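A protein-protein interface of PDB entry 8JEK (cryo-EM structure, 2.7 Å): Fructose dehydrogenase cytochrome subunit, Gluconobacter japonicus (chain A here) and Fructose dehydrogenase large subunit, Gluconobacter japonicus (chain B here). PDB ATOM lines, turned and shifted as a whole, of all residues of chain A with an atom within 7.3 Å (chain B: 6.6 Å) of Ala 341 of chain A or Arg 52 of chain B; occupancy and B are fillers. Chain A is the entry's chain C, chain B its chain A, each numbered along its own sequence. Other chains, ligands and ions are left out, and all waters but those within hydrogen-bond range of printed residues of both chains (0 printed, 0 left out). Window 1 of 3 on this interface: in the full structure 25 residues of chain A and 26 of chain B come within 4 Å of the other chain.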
ATOM      1  N   TYR A 315      -6.308   9.972  -7.034  1.00  0.00           N
ATOM      2  CA  TYR A 315      -5.002   9.457  -6.666  1.00  0.00           C
ATOM      3  C   TYR A 315      -4.976   9.110  -5.178  1.00  0.00           C
ATOM      4  O   TYR A 315      -5.986   9.201  -4.475  1.00  0.00           O
ATOM      5  CB  TYR A 315      -3.920  10.475  -7.049  1.00  0.00           C
ATOM      6  CG  TYR A 315      -3.586  11.512  -6.001  1.00  0.00           C
ATOM      7  CD1 TYR A 315      -4.579  12.244  -5.364  1.00  0.00           C
ATOM      8  CD2 TYR A 315      -2.264  11.774  -5.668  1.00  0.00           C
ATOM      9  CE1 TYR A 315      -4.264  13.188  -4.408  1.00  0.00           C
ATOM     10  CE2 TYR A 315      -1.941  12.715  -4.720  1.00  0.00           C
ATOM     11  CZ  TYR A 315      -2.943  13.419  -4.092  1.00  0.00           C
ATOM     12  OH  TYR A 315      -2.620  14.363  -3.145  1.00  0.00           O
ATOM     13  N   VAL A 317      -2.868  10.087  -1.701  1.00  0.00           N
ATOM     14  CA  VAL A 317      -1.894  10.962  -1.057  1.00  0.00           C
ATOM     15  C   VAL A 317      -0.841  10.142  -0.323  1.00  0.00           C
ATOM     16  O   VAL A 317       0.345  10.491  -0.320  1.00  0.00           O
ATOM     17  CB  VAL A 317      -2.604  11.946  -0.109  1.00  0.00           C
ATOM     18  CG1 VAL A 317      -1.681  13.093   0.261  1.00  0.00           C
ATOM     19  CG2 VAL A 317      -3.877  12.466  -0.743  1.00  0.00           C
ATOM     20  N   ASN A 321       4.094   9.508  -0.379  1.00  0.00           N
ATOM     21  CA  ASN A 321       5.132   9.700   0.627  1.00  0.00           C
ATOM     22  C   ASN A 321       6.420   8.976   0.272  1.00  0.00           C
ATOM     23  O   ASN A 321       7.494   9.387   0.722  1.00  0.00           O
ATOM     24  CB  ASN A 321       4.636   9.233   1.995  1.00  0.00           C
ATOM     25  CG  ASN A 321       3.367   9.927   2.421  1.00  0.00           C
ATOM     26  OD1 ASN A 321       3.256  11.147   2.333  1.00  0.00           O
ATOM     27  ND2 ASN A 321       2.401   9.153   2.892  1.00  0.00           N
ATOM     28  N   ARG A 324       8.742  11.344  -1.872  1.00  0.00           N
ATOM     29  CA  ARG A 324       9.460  12.460  -1.281  1.00  0.00           C
ATOM     30  C   ARG A 324      10.956  12.182  -1.334  1.00  0.00           C
ATOM     31  O   ARG A 324      11.391  11.028  -1.376  1.00  0.00           O
ATOM     32  CB  ARG A 324       9.000  12.697   0.156  1.00  0.00           C
ATOM     33  CG  ARG A 324       7.507  12.955   0.276  1.00  0.00           C
ATOM     34  CD  ARG A 324       7.114  13.342   1.685  1.00  0.00           C
ATOM     35  NE  ARG A 324       7.403  12.287   2.647  1.00  0.00           N
ATOM     36  CZ  ARG A 324       6.868  12.211   3.858  1.00  0.00           C
ATOM     37  NH1 ARG A 324       6.003  13.113   4.289  1.00  0.00           N
ATOM     38  NH2 ARG A 324       7.212  11.206   4.657  1.00  0.00           N
ATOM     39  N   LEU A 329      10.823  14.640 -10.984  1.00  0.00           N
ATOM     40  CA  LEU A 329       9.995  13.444 -11.094  1.00  0.00           C
ATOM     41  C   LEU A 329      10.303  12.595 -12.320  1.00  0.00           C
ATOM     42  O   LEU A 329      10.099  13.013 -13.462  1.00  0.00           O
ATOM     43  CB  LEU A 329       8.502  13.813 -11.092  1.00  0.00           C
ATOM     44  CG  LEU A 329       7.886  14.955 -11.913  1.00  0.00           C
ATOM     45  CD1 LEU A 329       7.473  14.532 -13.306  1.00  0.00           C
ATOM     46  CD2 LEU A 329       6.679  15.495 -11.180  1.00  0.00           C
ATOM     47  N   THR A 332       7.675   8.983 -10.852  1.00  0.00           N
ATOM     48  CA  THR A 332       6.243   9.256 -10.778  1.00  0.00           C
ATOM     49  C   THR A 332       5.633   8.832 -12.109  1.00  0.00           C
ATOM     50  O   THR A 332       5.342   9.659 -12.973  1.00  0.00           O
ATOM     51  CB  THR A 332       5.978  10.728 -10.484  1.00  0.00           C
ATOM     52  OG1 THR A 332       6.906  11.196  -9.499  1.00  0.00           O
ATOM     53  CG2 THR A 332       4.562  10.922  -9.971  1.00  0.00           C
ATOM     54  N   GLY A 335      -0.424   7.733 -13.488  1.00  0.00           N
ATOM     55  CA  GLY A 335      -1.177   8.770 -14.172  1.00  0.00           C
ATOM     56  C   GLY A 335      -1.923   9.681 -13.218  1.00  0.00           C
ATOM     57  O   GLY A 335      -1.996  10.894 -13.433  1.00  0.00           O
ATOM     58  N   ALA A 336      -2.495   9.110 -12.157  1.00  0.00           N
ATOM     59  CA  ALA A 336      -3.211   9.917 -11.175  1.00  0.00           C
ATOM     60  C   ALA A 336      -2.271  10.868 -10.447  1.00  0.00           C
ATOM     61  O   ALA A 336      -2.593  12.048 -10.261  1.00  0.00           O
ATOM     62  CB  ALA A 336      -3.933   9.008 -10.185  1.00  0.00           C
ATOM     63  N   ALA A 337      -1.098  10.376 -10.041  1.00  0.00           N
ATOM     64  CA  ALA A 337      -0.125  11.230  -9.370  1.00  0.00           C
ATOM     65  C   ALA A 337       0.390  12.317 -10.302  1.00  0.00           C
ATOM     66  O   ALA A 337       0.592  13.462  -9.882  1.00  0.00           O
ATOM     67  CB  ALA A 337       1.030  10.387  -8.836  1.00  0.00           C
ATOM     68  N   LEU A 338       0.623  11.976 -11.571  1.00  0.00           N
ATOM     69  CA  LEU A 338       1.083  12.967 -12.535  1.00  0.00           C
ATOM     70  C   LEU A 338       0.030  14.044 -12.773  1.00  0.00           C
ATOM     71  O   LEU A 338       0.358  15.234 -12.843  1.00  0.00           O
ATOM     72  CB  LEU A 338       1.461  12.281 -13.846  1.00  0.00           C
ATOM     73  CG  LEU A 338       2.837  11.617 -13.913  1.00  0.00           C
ATOM     74  CD1 LEU A 338       2.911  10.667 -15.093  1.00  0.00           C
ATOM     75  CD2 LEU A 338       3.937  12.659 -13.997  1.00  0.00           C
ATOM     76  N   TYR A 339      -1.239  13.648 -12.896  1.00  0.00           N
ATOM     77  CA  TYR A 339      -2.306  14.635 -13.024  1.00  0.00           C
ATOM     78  C   TYR A 339      -2.378  15.522 -11.791  1.00  0.00           C
ATOM     79  O   TYR A 339      -2.564  16.738 -11.903  1.00  0.00           O
ATOM     80  CB  TYR A 339      -3.651  13.946 -13.262  1.00  0.00           C
ATOM     81  CG  TYR A 339      -4.836  14.890 -13.169  1.00  0.00           C
ATOM     82  CD1 TYR A 339      -5.256  15.619 -14.271  1.00  0.00           C
ATOM     83  CD2 TYR A 339      -5.528  15.053 -11.978  1.00  0.00           C
ATOM     84  CE1 TYR A 339      -6.327  16.486 -14.187  1.00  0.00           C
ATOM     85  CE2 TYR A 339      -6.596  15.916 -11.886  1.00  0.00           C
ATOM     86  CZ  TYR A 339      -6.993  16.628 -12.991  1.00  0.00           C
ATOM     87  OH  TYR A 339      -8.062  17.485 -12.895  1.00  0.00           O
ATOM     88  N   GLU A 340      -2.245  14.931 -10.603  1.00  0.00           N
ATOM     89  CA  GLU A 340      -2.320  15.720  -9.380  1.00  0.00           C
ATOM     90  C   GLU A 340      -1.173  16.716  -9.289  1.00  0.00           C
ATOM     91  O   GLU A 340      -1.367  17.860  -8.863  1.00  0.00           O
ATOM     92  CB  GLU A 340      -2.333  14.802  -8.163  1.00  0.00           C
ATOM     93  CG  GLU A 340      -2.747  15.497  -6.884  1.00  0.00           C
ATOM     94  CD  GLU A 340      -4.242  15.687  -6.786  1.00  0.00           C
ATOM     95  OE1 GLU A 340      -4.976  15.060  -7.576  1.00  0.00           O
ATOM     96  OE2 GLU A 340      -4.686  16.462  -5.916  1.00  0.00           O
ATOM     97  N   ALA A 341       0.030  16.299  -9.679  1.00  0.00           N
ATOM     98  CA  ALA A 341       1.188  17.172  -9.551  1.00  0.00           C
ATOM     99  C   ALA A 341       1.180  18.274 -10.602  1.00  0.00           C
ATOM    100  O   ALA A 341       1.542  19.418 -10.308  1.00  0.00           O
ATOM    101  CB  ALA A 341       2.473  16.352  -9.643  1.00  0.00           C
ATOM    102  N   VAL A 342       0.768  17.958 -11.829  1.00  0.00           N
ATOM    103  CA  VAL A 342       0.918  18.900 -12.932  1.00  0.00           C
ATOM    104  C   VAL A 342      -0.378  19.654 -13.207  1.00  0.00           C
ATOM    105  O   VAL A 342      -0.353  20.849 -13.521  1.00  0.00           O
ATOM    106  CB  VAL A 342       1.410  18.182 -14.202  1.00  0.00           C
ATOM    107  CG1 VAL A 342       1.774  19.189 -15.273  1.00  0.00           C
ATOM    108  CG2 VAL A 342       2.604  17.304 -13.883  1.00  0.00           C
ATOM    109  N   CYS A 343      -1.516  18.976 -13.085  1.00  0.00           N
ATOM    110  CA  CYS A 343      -2.773  19.515 -13.586  1.00  0.00           C
ATOM    111  C   CYS A 343      -3.798  19.852 -12.513  1.00  0.00           C
ATOM    112  O   CYS A 343      -4.673  20.679 -12.770  1.00  0.00           O
ATOM    113  CB  CYS A 343      -3.415  18.528 -14.573  1.00  0.00           C
ATOM    114  SG  CYS A 343      -2.256  17.684 -15.671  1.00  0.00           S
ATOM    115  N   ALA A 344      -3.719  19.250 -11.327  1.00  0.00           N
ATOM    116  CA  ALA A 344      -4.804  19.356 -10.358  1.00  0.00           C
ATOM    117  C   ALA A 344      -4.882  20.709  -9.660  1.00  0.00           C
ATOM    118  O   ALA A 344      -5.850  20.948  -8.931  1.00  0.00           O
ATOM    119  CB  ALA A 344      -4.692  18.259  -9.304  1.00  0.00           C
ATOM    120  N   SER A 345      -3.900  21.591  -9.843  1.00  0.00           N
ATOM    121  CA  SER A 345      -3.968  22.895  -9.194  1.00  0.00           C
ATOM    122  C   SER A 345      -5.113  23.733  -9.748  1.00  0.00           C
ATOM    123  O   SER A 345      -5.836  24.385  -8.987  1.00  0.00           O
ATOM    124  CB  SER A 345      -2.640  23.631  -9.353  1.00  0.00           C
ATOM    125  OG  SER A 345      -2.750  24.970  -8.909  1.00  0.00           O
ATOM    126  N   CYS A 346      -5.292  23.729 -11.069  1.00  0.00           N
ATOM    127  CA  CYS A 346      -6.304  24.556 -11.719  1.00  0.00           C
ATOM    128  C   CYS A 346      -7.595  23.783 -11.972  1.00  0.00           C
ATOM    129  O   CYS A 346      -8.658  24.159 -11.471  1.00  0.00           O
ATOM    130  CB  CYS A 346      -5.734  25.118 -13.020  1.00  0.00           C
ATOM    131  SG  CYS A 346      -4.281  26.122 -12.729  1.00  0.00           S
ATOM    132  N   GLN A 405       6.513  23.241 -16.667  1.00  0.00           N
ATOM    133  CA  GLN A 405       6.805  21.845 -16.375  1.00  0.00           C
ATOM    134  C   GLN A 405       6.952  21.064 -17.674  1.00  0.00           C
ATOM    135  O   GLN A 405       5.954  20.587 -18.229  1.00  0.00           O
ATOM    136  CB  GLN A 405       5.711  21.233 -15.500  1.00  0.00           C
ATOM    137  CG  GLN A 405       5.952  19.779 -15.130  1.00  0.00           C
ATOM    138  CD  GLN A 405       7.345  19.534 -14.590  1.00  0.00           C
ATOM    139  OE1 GLN A 405       7.684  19.975 -13.497  1.00  0.00           O
ATOM    140  NE2 GLN A 405       8.158  18.821 -15.357  1.00  0.00           N
ATOM    141  N   ILE A 415      -0.778  11.008 -18.514  1.00  0.00           N
ATOM    142  CA  ILE A 415      -1.740  11.989 -18.016  1.00  0.00           C
ATOM    143  C   ILE A 415      -2.996  11.993 -18.878  1.00  0.00           C
ATOM    144  O   ILE A 415      -4.120  12.054 -18.363  1.00  0.00           O
ATOM    145  CB  ILE A 415      -1.095  13.385 -17.943  1.00  0.00           C
ATOM    146  CG1 ILE A 415       0.014  13.404 -16.892  1.00  0.00           C
ATOM    147  CG2 ILE A 415      -2.138  14.439 -17.620  1.00  0.00           C
ATOM    148  CD1 ILE A 415       0.759  14.712 -16.812  1.00  0.00           C
ATOM    149  N   ARG B  44       9.204  21.331 -11.124  1.00  0.00           N
ATOM    150  CA  ARG B  44       8.261  22.122 -10.340  1.00  0.00           C
ATOM    151  C   ARG B  44       7.165  21.248  -9.749  1.00  0.00           C
ATOM    152  O   ARG B  44       6.813  21.391  -8.572  1.00  0.00           O
ATOM    153  CB  ARG B  44       7.656  23.220 -11.212  1.00  0.00           C
ATOM    154  CG  ARG B  44       6.336  23.758 -10.709  1.00  0.00           C
ATOM    155  CD  ARG B  44       5.821  24.850 -11.617  1.00  0.00           C
ATOM    156  NE  ARG B  44       6.912  25.576 -12.255  1.00  0.00           N
ATOM    157  CZ  ARG B  44       7.405  26.724 -11.815  1.00  0.00           C
ATOM    158  NH1 ARG B  44       6.923  27.315 -10.736  1.00  0.00           N
ATOM    159  NH2 ARG B  44       8.411  27.291 -12.474  1.00  0.00           N
ATOM    160  N   SER B  45       6.620  20.331 -10.545  1.00  0.00           N
ATOM    161  CA  SER B  45       5.546  19.462 -10.087  1.00  0.00           C
ATOM    162  C   SER B  45       5.994  18.483  -9.013  1.00  0.00           C
ATOM    163  O   SER B  45       5.211  18.179  -8.108  1.00  0.00           O
ATOM    164  CB  SER B  45       4.954  18.701 -11.272  1.00  0.00           C
ATOM    165  OG  SER B  45       4.438  19.601 -12.234  1.00  0.00           O
ATOM    166  N   GLN B  46       7.231  17.996  -9.076  1.00  0.00           N
ATOM    167  CA  GLN B  46       7.757  17.155  -8.011  1.00  0.00           C
ATOM    168  C   GLN B  46       7.922  17.919  -6.704  1.00  0.00           C
ATOM    169  O   GLN B  46       7.610  17.386  -5.638  1.00  0.00           O
ATOM    170  CB  GLN B  46       9.090  16.537  -8.432  1.00  0.00           C
ATOM    171  CG  GLN B  46       9.600  15.472  -7.477  1.00  0.00           C
ATOM    172  CD  GLN B  46       8.536  14.465  -7.080  1.00  0.00           C
ATOM    173  OE1 GLN B  46       8.021  13.727  -7.914  1.00  0.00           O
ATOM    174  NE2 GLN B  46       8.218  14.418  -5.794  1.00  0.00           N
ATOM    175  N   ILE B  47       8.402  19.163  -6.762  1.00  0.00           N
ATOM    176  CA  ILE B  47       8.485  19.973  -5.551  1.00  0.00           C
ATOM    177  C   ILE B  47       7.095  20.270  -5.012  1.00  0.00           C
ATOM    178  O   ILE B  47       6.891  20.327  -3.793  1.00  0.00           O
ATOM    179  CB  ILE B  47       9.275  21.270  -5.817  1.00  0.00           C
ATOM    180  CG1 ILE B  47      10.639  20.963  -6.442  1.00  0.00           C
ATOM    181  CG2 ILE B  47       9.441  22.065  -4.537  1.00  0.00           C
ATOM    182  CD1 ILE B  47      11.406  19.839  -5.767  1.00  0.00           C
ATOM    183  N   VAL B  48       6.120  20.469  -5.900  1.00  0.00           N
ATOM    184  CA  VAL B  48       4.745  20.690  -5.464  1.00  0.00           C
ATOM    185  C   VAL B  48       4.209  19.462  -4.738  1.00  0.00           C
ATOM    186  O   VAL B  48       3.584  19.574  -3.675  1.00  0.00           O
ATOM    187  CB  VAL B  48       3.871  21.068  -6.673  1.00  0.00           C
ATOM    188  CG1 VAL B  48       2.408  20.896  -6.350  1.00  0.00           C
ATOM    189  CG2 VAL B  48       4.160  22.490  -7.099  1.00  0.00           C
ATOM    190  N   GLU B  49       4.454  18.274  -5.293  1.00  0.00           N
ATOM    191  CA  GLU B  49       4.049  17.038  -4.630  1.00  0.00           C
ATOM    192  C   GLU B  49       4.755  16.872  -3.291  1.00  0.00           C
ATOM    193  O   GLU B  49       4.146  16.430  -2.310  1.00  0.00           O
ATOM    194  CB  GLU B  49       4.337  15.844  -5.536  1.00  0.00           C
ATOM    195  CG  GLU B  49       3.833  14.520  -4.995  1.00  0.00           C
ATOM    196  CD  GLU B  49       4.090  13.371  -5.945  1.00  0.00           C
ATOM    197  OE1 GLU B  49       4.941  13.524  -6.844  1.00  0.00           O
ATOM    198  OE2 GLU B  49       3.436  12.318  -5.801  1.00  0.00           O
ATOM    199  N   ASN B  50       6.045  17.210  -3.235  1.00  0.00           N
ATOM    200  CA  ASN B  50       6.812  17.103  -2.000  1.00  0.00           C
ATOM    201  C   ASN B  50       6.310  18.048  -0.920  1.00  0.00           C
ATOM    202  O   ASN B  50       6.299  17.670   0.255  1.00  0.00           O
ATOM    203  CB  ASN B  50       8.290  17.379  -2.276  1.00  0.00           C
ATOM    204  CG  ASN B  50       8.948  16.282  -3.079  1.00  0.00           C
ATOM    205  OD1 ASN B  50       8.316  15.288  -3.426  1.00  0.00           O
ATOM    206  ND2 ASN B  50      10.225  16.460  -3.386  1.00  0.00           N
ATOM    207  N   TRP B  51       5.913  19.267  -1.283  1.00  0.00           N
ATOM    208  CA  TRP B  51       5.326  20.179  -0.311  1.00  0.00           C
ATOM    209  C   TRP B  51       3.938  19.734   0.122  1.00  0.00           C
ATOM    210  O   TRP B  51       3.588  19.870   1.296  1.00  0.00           O
ATOM    211  CB  TRP B  51       5.248  21.602  -0.870  1.00  0.00           C
ATOM    212  CG  TRP B  51       4.643  22.576   0.106  1.00  0.00           C
ATOM    213  CD1 TRP B  51       5.302  23.288   1.060  1.00  0.00           C
ATOM    214  CD2 TRP B  51       3.259  22.926   0.231  1.00  0.00           C
ATOM    215  NE1 TRP B  51       4.421  24.065   1.768  1.00  0.00           N
ATOM    216  CE2 TRP B  51       3.159  23.860   1.279  1.00  0.00           C
ATOM    217  CE3 TRP B  51       2.095  22.541  -0.439  1.00  0.00           C
ATOM    218  CZ2 TRP B  51       1.944  24.415   1.668  1.00  0.00           C
ATOM    219  CZ3 TRP B  51       0.894  23.093  -0.051  1.00  0.00           C
ATOM    220  CH2 TRP B  51       0.826  24.017   0.992  1.00  0.00           C
ATOM    221  N   ARG B  52       3.135  19.210  -0.807  1.00  0.00           N
ATOM    222  CA  ARG B  52       1.804  18.739  -0.442  1.00  0.00           C
ATOM    223  C   ARG B  52       1.869  17.584   0.546  1.00  0.00           C
ATOM    224  O   ARG B  52       1.021  17.482   1.439  1.00  0.00           O
ATOM    225  CB  ARG B  52       1.029  18.327  -1.693  1.00  0.00           C
ATOM    226  CG  ARG B  52       0.519  19.488  -2.517  1.00  0.00           C
ATOM    227  CD  ARG B  52       0.185  19.059  -3.930  1.00  0.00           C
ATOM    228  NE  ARG B  52      -0.445  20.131  -4.688  1.00  0.00           N
ATOM    229  CZ  ARG B  52      -0.856  20.022  -5.943  1.00  0.00           C
ATOM    230  NH1 ARG B  52      -0.721  18.893  -6.617  1.00  0.00           N
ATOM    231  NH2 ARG B  52      -1.420  21.070  -6.535  1.00  0.00           N
ATOM    232  N   ASN B  53       2.865  16.712   0.410  1.00  0.00           N
ATOM    233  CA  ASN B  53       3.067  15.597   1.321  1.00  0.00           C
ATOM    234  C   ASN B  53       3.999  15.944   2.473  1.00  0.00           C
ATOM    235  O   ASN B  53       4.368  15.057   3.246  1.00  0.00           O
ATOM    236  CB  ASN B  53       3.600  14.388   0.555  1.00  0.00           C
ATOM    237  CG  ASN B  53       2.493  13.548  -0.037  1.00  0.00           C
ATOM    238  OD1 ASN B  53       2.144  13.698  -1.204  1.00  0.00           O
ATOM    239  ND2 ASN B  53       1.932  12.655   0.768  1.00  0.00           N
ATOM    240  N   MET B  54       4.400  17.196   2.586  1.00  0.00           N
ATOM    241  CA  MET B  54       5.130  17.706   3.735  1.00  0.00           C
ATOM    242  C   MET B  54       4.177  17.870   4.918  1.00  0.00           C
ATOM    243  O   MET B  54       3.044  18.322   4.739  1.00  0.00           O
ATOM    244  CB  MET B  54       5.793  19.036   3.379  1.00  0.00           C
ATOM    245  CG  MET B  54       7.108  19.319   4.076  1.00  0.00           C
ATOM    246  SD  MET B  54       7.576  21.051   3.924  1.00  0.00           S
ATOM    247  CE  MET B  54       6.076  21.860   4.443  1.00  0.00           C
ATOM    248  N   PRO B  55       4.602  17.501   6.123  1.00  0.00           N
ATOM    249  CA  PRO B  55       3.682  17.459   7.268  1.00  0.00           C
ATOM    250  C   PRO B  55       3.084  18.823   7.560  1.00  0.00           C
ATOM    251  O   PRO B  55       3.709  19.859   7.294  1.00  0.00           O
ATOM    252  CB  PRO B  55       4.579  16.986   8.419  1.00  0.00           C
ATOM    253  CG  PRO B  55       5.635  16.194   7.750  1.00  0.00           C
ATOM    254  CD  PRO B  55       5.901  16.886   6.446  1.00  0.00           C
ATOM    255  N   LYS B  59       4.216  23.035   7.440  1.00  0.00           N
ATOM    256  CA  LYS B  59       3.517  24.082   6.708  1.00  0.00           C
ATOM    257  C   LYS B  59       3.128  25.239   7.617  1.00  0.00           C
ATOM    258  O   LYS B  59       3.203  26.402   7.206  1.00  0.00           O
ATOM    259  CB  LYS B  59       2.268  23.515   6.031  1.00  0.00           C
ATOM    260  CG  LYS B  59       2.536  22.512   4.929  1.00  0.00           C
ATOM    261  CD  LYS B  59       1.237  21.904   4.431  1.00  0.00           C
ATOM    262  CE  LYS B  59       1.484  20.872   3.353  1.00  0.00           C
ATOM    263  NZ  LYS B  59       0.764  19.601   3.624  1.00  0.00           N
ATOM    264  N   PRO B  67      10.698  20.595   0.775  1.00  0.00           N
ATOM    265  CA  PRO B  67      10.278  20.131  -0.557  1.00  0.00           C
ATOM    266  C   PRO B  67      11.418  19.982  -1.546  1.00  0.00           C
ATOM    267  O   PRO B  67      11.258  19.273  -2.546  1.00  0.00           O
ATOM    268  CB  PRO B  67       9.288  21.212  -1.004  1.00  0.00           C
ATOM    269  CG  PRO B  67       8.756  21.758   0.256  1.00  0.00           C
ATOM    270  CD  PRO B  67       9.919  21.777   1.189  1.00  0.00           C
ATOM    271  N   ASN B 219      -2.643  30.999  -5.575  1.00  0.00           N
ATOM    272  CA  ASN B 219      -2.311  29.744  -4.912  1.00  0.00           C
ATOM    273  C   ASN B 219      -1.649  29.964  -3.558  1.00  0.00           C
ATOM    274  O   ASN B 219      -1.602  29.035  -2.753  1.00  0.00           O
ATOM    275  CB  ASN B 219      -1.405  28.893  -5.799  1.00  0.00           C
ATOM    276  CG  ASN B 219      -2.182  28.033  -6.773  1.00  0.00           C
ATOM    277  OD1 ASN B 219      -1.880  27.994  -7.962  1.00  0.00           O
ATOM    278  ND2 ASN B 219      -3.188  27.339  -6.271  1.00  0.00           N
ATOM    279  N   ILE B 225       6.846  26.900  -3.321  1.00  0.00           N
ATOM    280  CA  ILE B 225       6.738  26.492  -4.719  1.00  0.00           C
ATOM    281  C   ILE B 225       5.396  26.902  -5.317  1.00  0.00           C
ATOM    282  O   ILE B 225       4.338  26.675  -4.724  1.00  0.00           O
ATOM    283  CB  ILE B 225       6.979  24.975  -4.871  1.00  0.00           C
ATOM    284  CG1 ILE B 225       7.020  24.576  -6.348  1.00  0.00           C
ATOM    285  CG2 ILE B 225       5.956  24.161  -4.084  1.00  0.00           C
ATOM    286  CD1 ILE B 225       8.208  25.122  -7.095  1.00  0.00           C
ATOM    287  N   PRO B 227       2.645  26.144  -8.055  1.00  0.00           N
ATOM    288  CA  PRO B 227       2.289  24.966  -8.860  1.00  0.00           C
ATOM    289  C   PRO B 227       2.102  25.259 -10.335  1.00  0.00           C
ATOM    290  O   PRO B 227       2.251  24.341 -11.150  1.00  0.00           O
ATOM    291  CB  PRO B 227       0.976  24.481  -8.227  1.00  0.00           C
ATOM    292  CG  PRO B 227       0.754  25.330  -7.016  1.00  0.00           C
ATOM    293  CD  PRO B 227       1.539  26.576  -7.189  1.00  0.00           C
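N of Ser 45 of chain B lies within hydrogen-bond range of OE1 of Gln 405 of chain A (3.2 Å).
The side-chain amide oxygen of Asn 219 of chain B sits at hydrogen-bond distance from the side-chain hydroxyl of Ser 345 of chain A (3.3 Å).
The backbone NH of Arg 44 of chain B lies within hydrogen-bond range of the side-chain amide oxygen of Gln 405 of chain A (3.1 Å).
The backbone carbonyl oxygen (O) of Val 317 of chain A lies within hydrogen-bond range of the side-chain amide nitrogen (ND2) of Asn 53 of chain B, at 2.9 Å.
The side-chain hydroxyl (OG) of Ser 45 of chain B lies within hydrogen-bond range of the backbone carbonyl oxygen (O) of Ala 341 of chain A.
The side-chain amide nitrogen (ND2) of Asn 53 of chain B lies within hydrogen-bond range of the side-chain amide oxygen (OD1) of Asn 321 of chain A (2.5 Å).
The side-chain hydroxyl of Thr 332 of chain A sits at hydrogen-bond distance from the side-chain amide oxygen of Gln 46 of chain B (3.2 Å).
NH1 of Arg 52 of chain B lies within hydrogen-bond range of O of Glu 340 of chain A.
O of Asn 53 of chain B lies within hydrogen-bond range of NH1 of Arg 324 of chain A (2.7 Å).
The backbone carbonyl oxygen (O) of Pro 67 of chain B lies within hydrogen-bond range of the side-chain amide nitrogen (ND2) of Asn 50 of chain B, 3.1 Å away.
NE2 of Gln 46 of chain B sits at hydrogen-bond distance from OD1 of Asn 50 of chain B.
O of Asn 321 of chain A is in hydrogen-bond range of NE of Arg 324 of chain A (3.5 Å).
The side-chain carboxylate (OE1) of Glu 49 of chain B sits close to the side-chain amide oxygen (OE1) of Gln 46 of chain B (3.3 Å).
The backbone carbonyl oxygen (O) of Arg 52 of chain B is in hydrogen-bond range of the side-chain amino group (NZ) of Lys 59 of chain B (3.1 Å).
Among the printed residues, merely in contact across the chains: Arg 324 of chain A with Asn 50 of chain B (3.7 Å), Leu 329 of chain A with Ser 45 of chain B (3.6 Å), Leu 329 of chain A with Gln 46 of chain B (3.2 Å), Ala 341 of chain A with Arg 52 of chain B (3.9 Å), Val 342 of chain A with Ser 45 of chain B (3.4 Å), Ser 345 of chain A with Arg 52 of chain B (3.999 Å) and Ser 345 of chain A with Pro 227 of chain B (3.8 Å).
Of the printed residues of chain B, Asn 321 of chain A touches Asn 53.
Of the printed residues of chain B, Arg 324 of chain A touches Asn 50 (3.7 Å) and Asn 53 (2.7 Å).
Of chain B, only Ser 45 and Arg 52 come within 4 Å of Ala 341 of chain A.
Of the printed residues of chain B, Ser 345 of chain A touches Arg 52 (3.999 Å), Asn 219 (3.3 Å) and Pro 227 (3.8 Å).
Cys 346 of chain A touches none of the printed residues of chain B.
Printed residues of chain A within 4 Å of Arg 52 of chain B: Glu 340 (2.6 Å), Ala 341 (3.9 Å) and Ser 345 (3.999 Å).
The nearest residue of chain B that does not touch Ala 341 of chain A is Val 48 of chain B (4.3 Å).
The nearest printed residue of chain A that does not touch Arg 44 of chain B is Ala 341 of chain A (5.9 Å).
Of the 17 printed residues of chain B, 8 touch a printed residue of chain A.
Printed residues of chain B that touch a printed residue of chain A: Arg 44, Ser 45, Gln 46, Asn 50, Arg 52, Asn 53, Asn 219 and Pro 227.
Hydrophobic or aromatic side chains of chain B that line the printed part of chain A: Pro 227.
Of the 20 printed residues of chain A, 10 touch a printed residue of chain B.
Printed residues of chain A that touch a printed residue of chain B: Val 317, Asn 321, Arg 324, Leu 329, Thr 332, Glu 340, Ala 341, Val 342, Ser 345 and Gln 405.
Along chain A the printed residues that touch a printed residue of chain B span positions 317 to 405.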
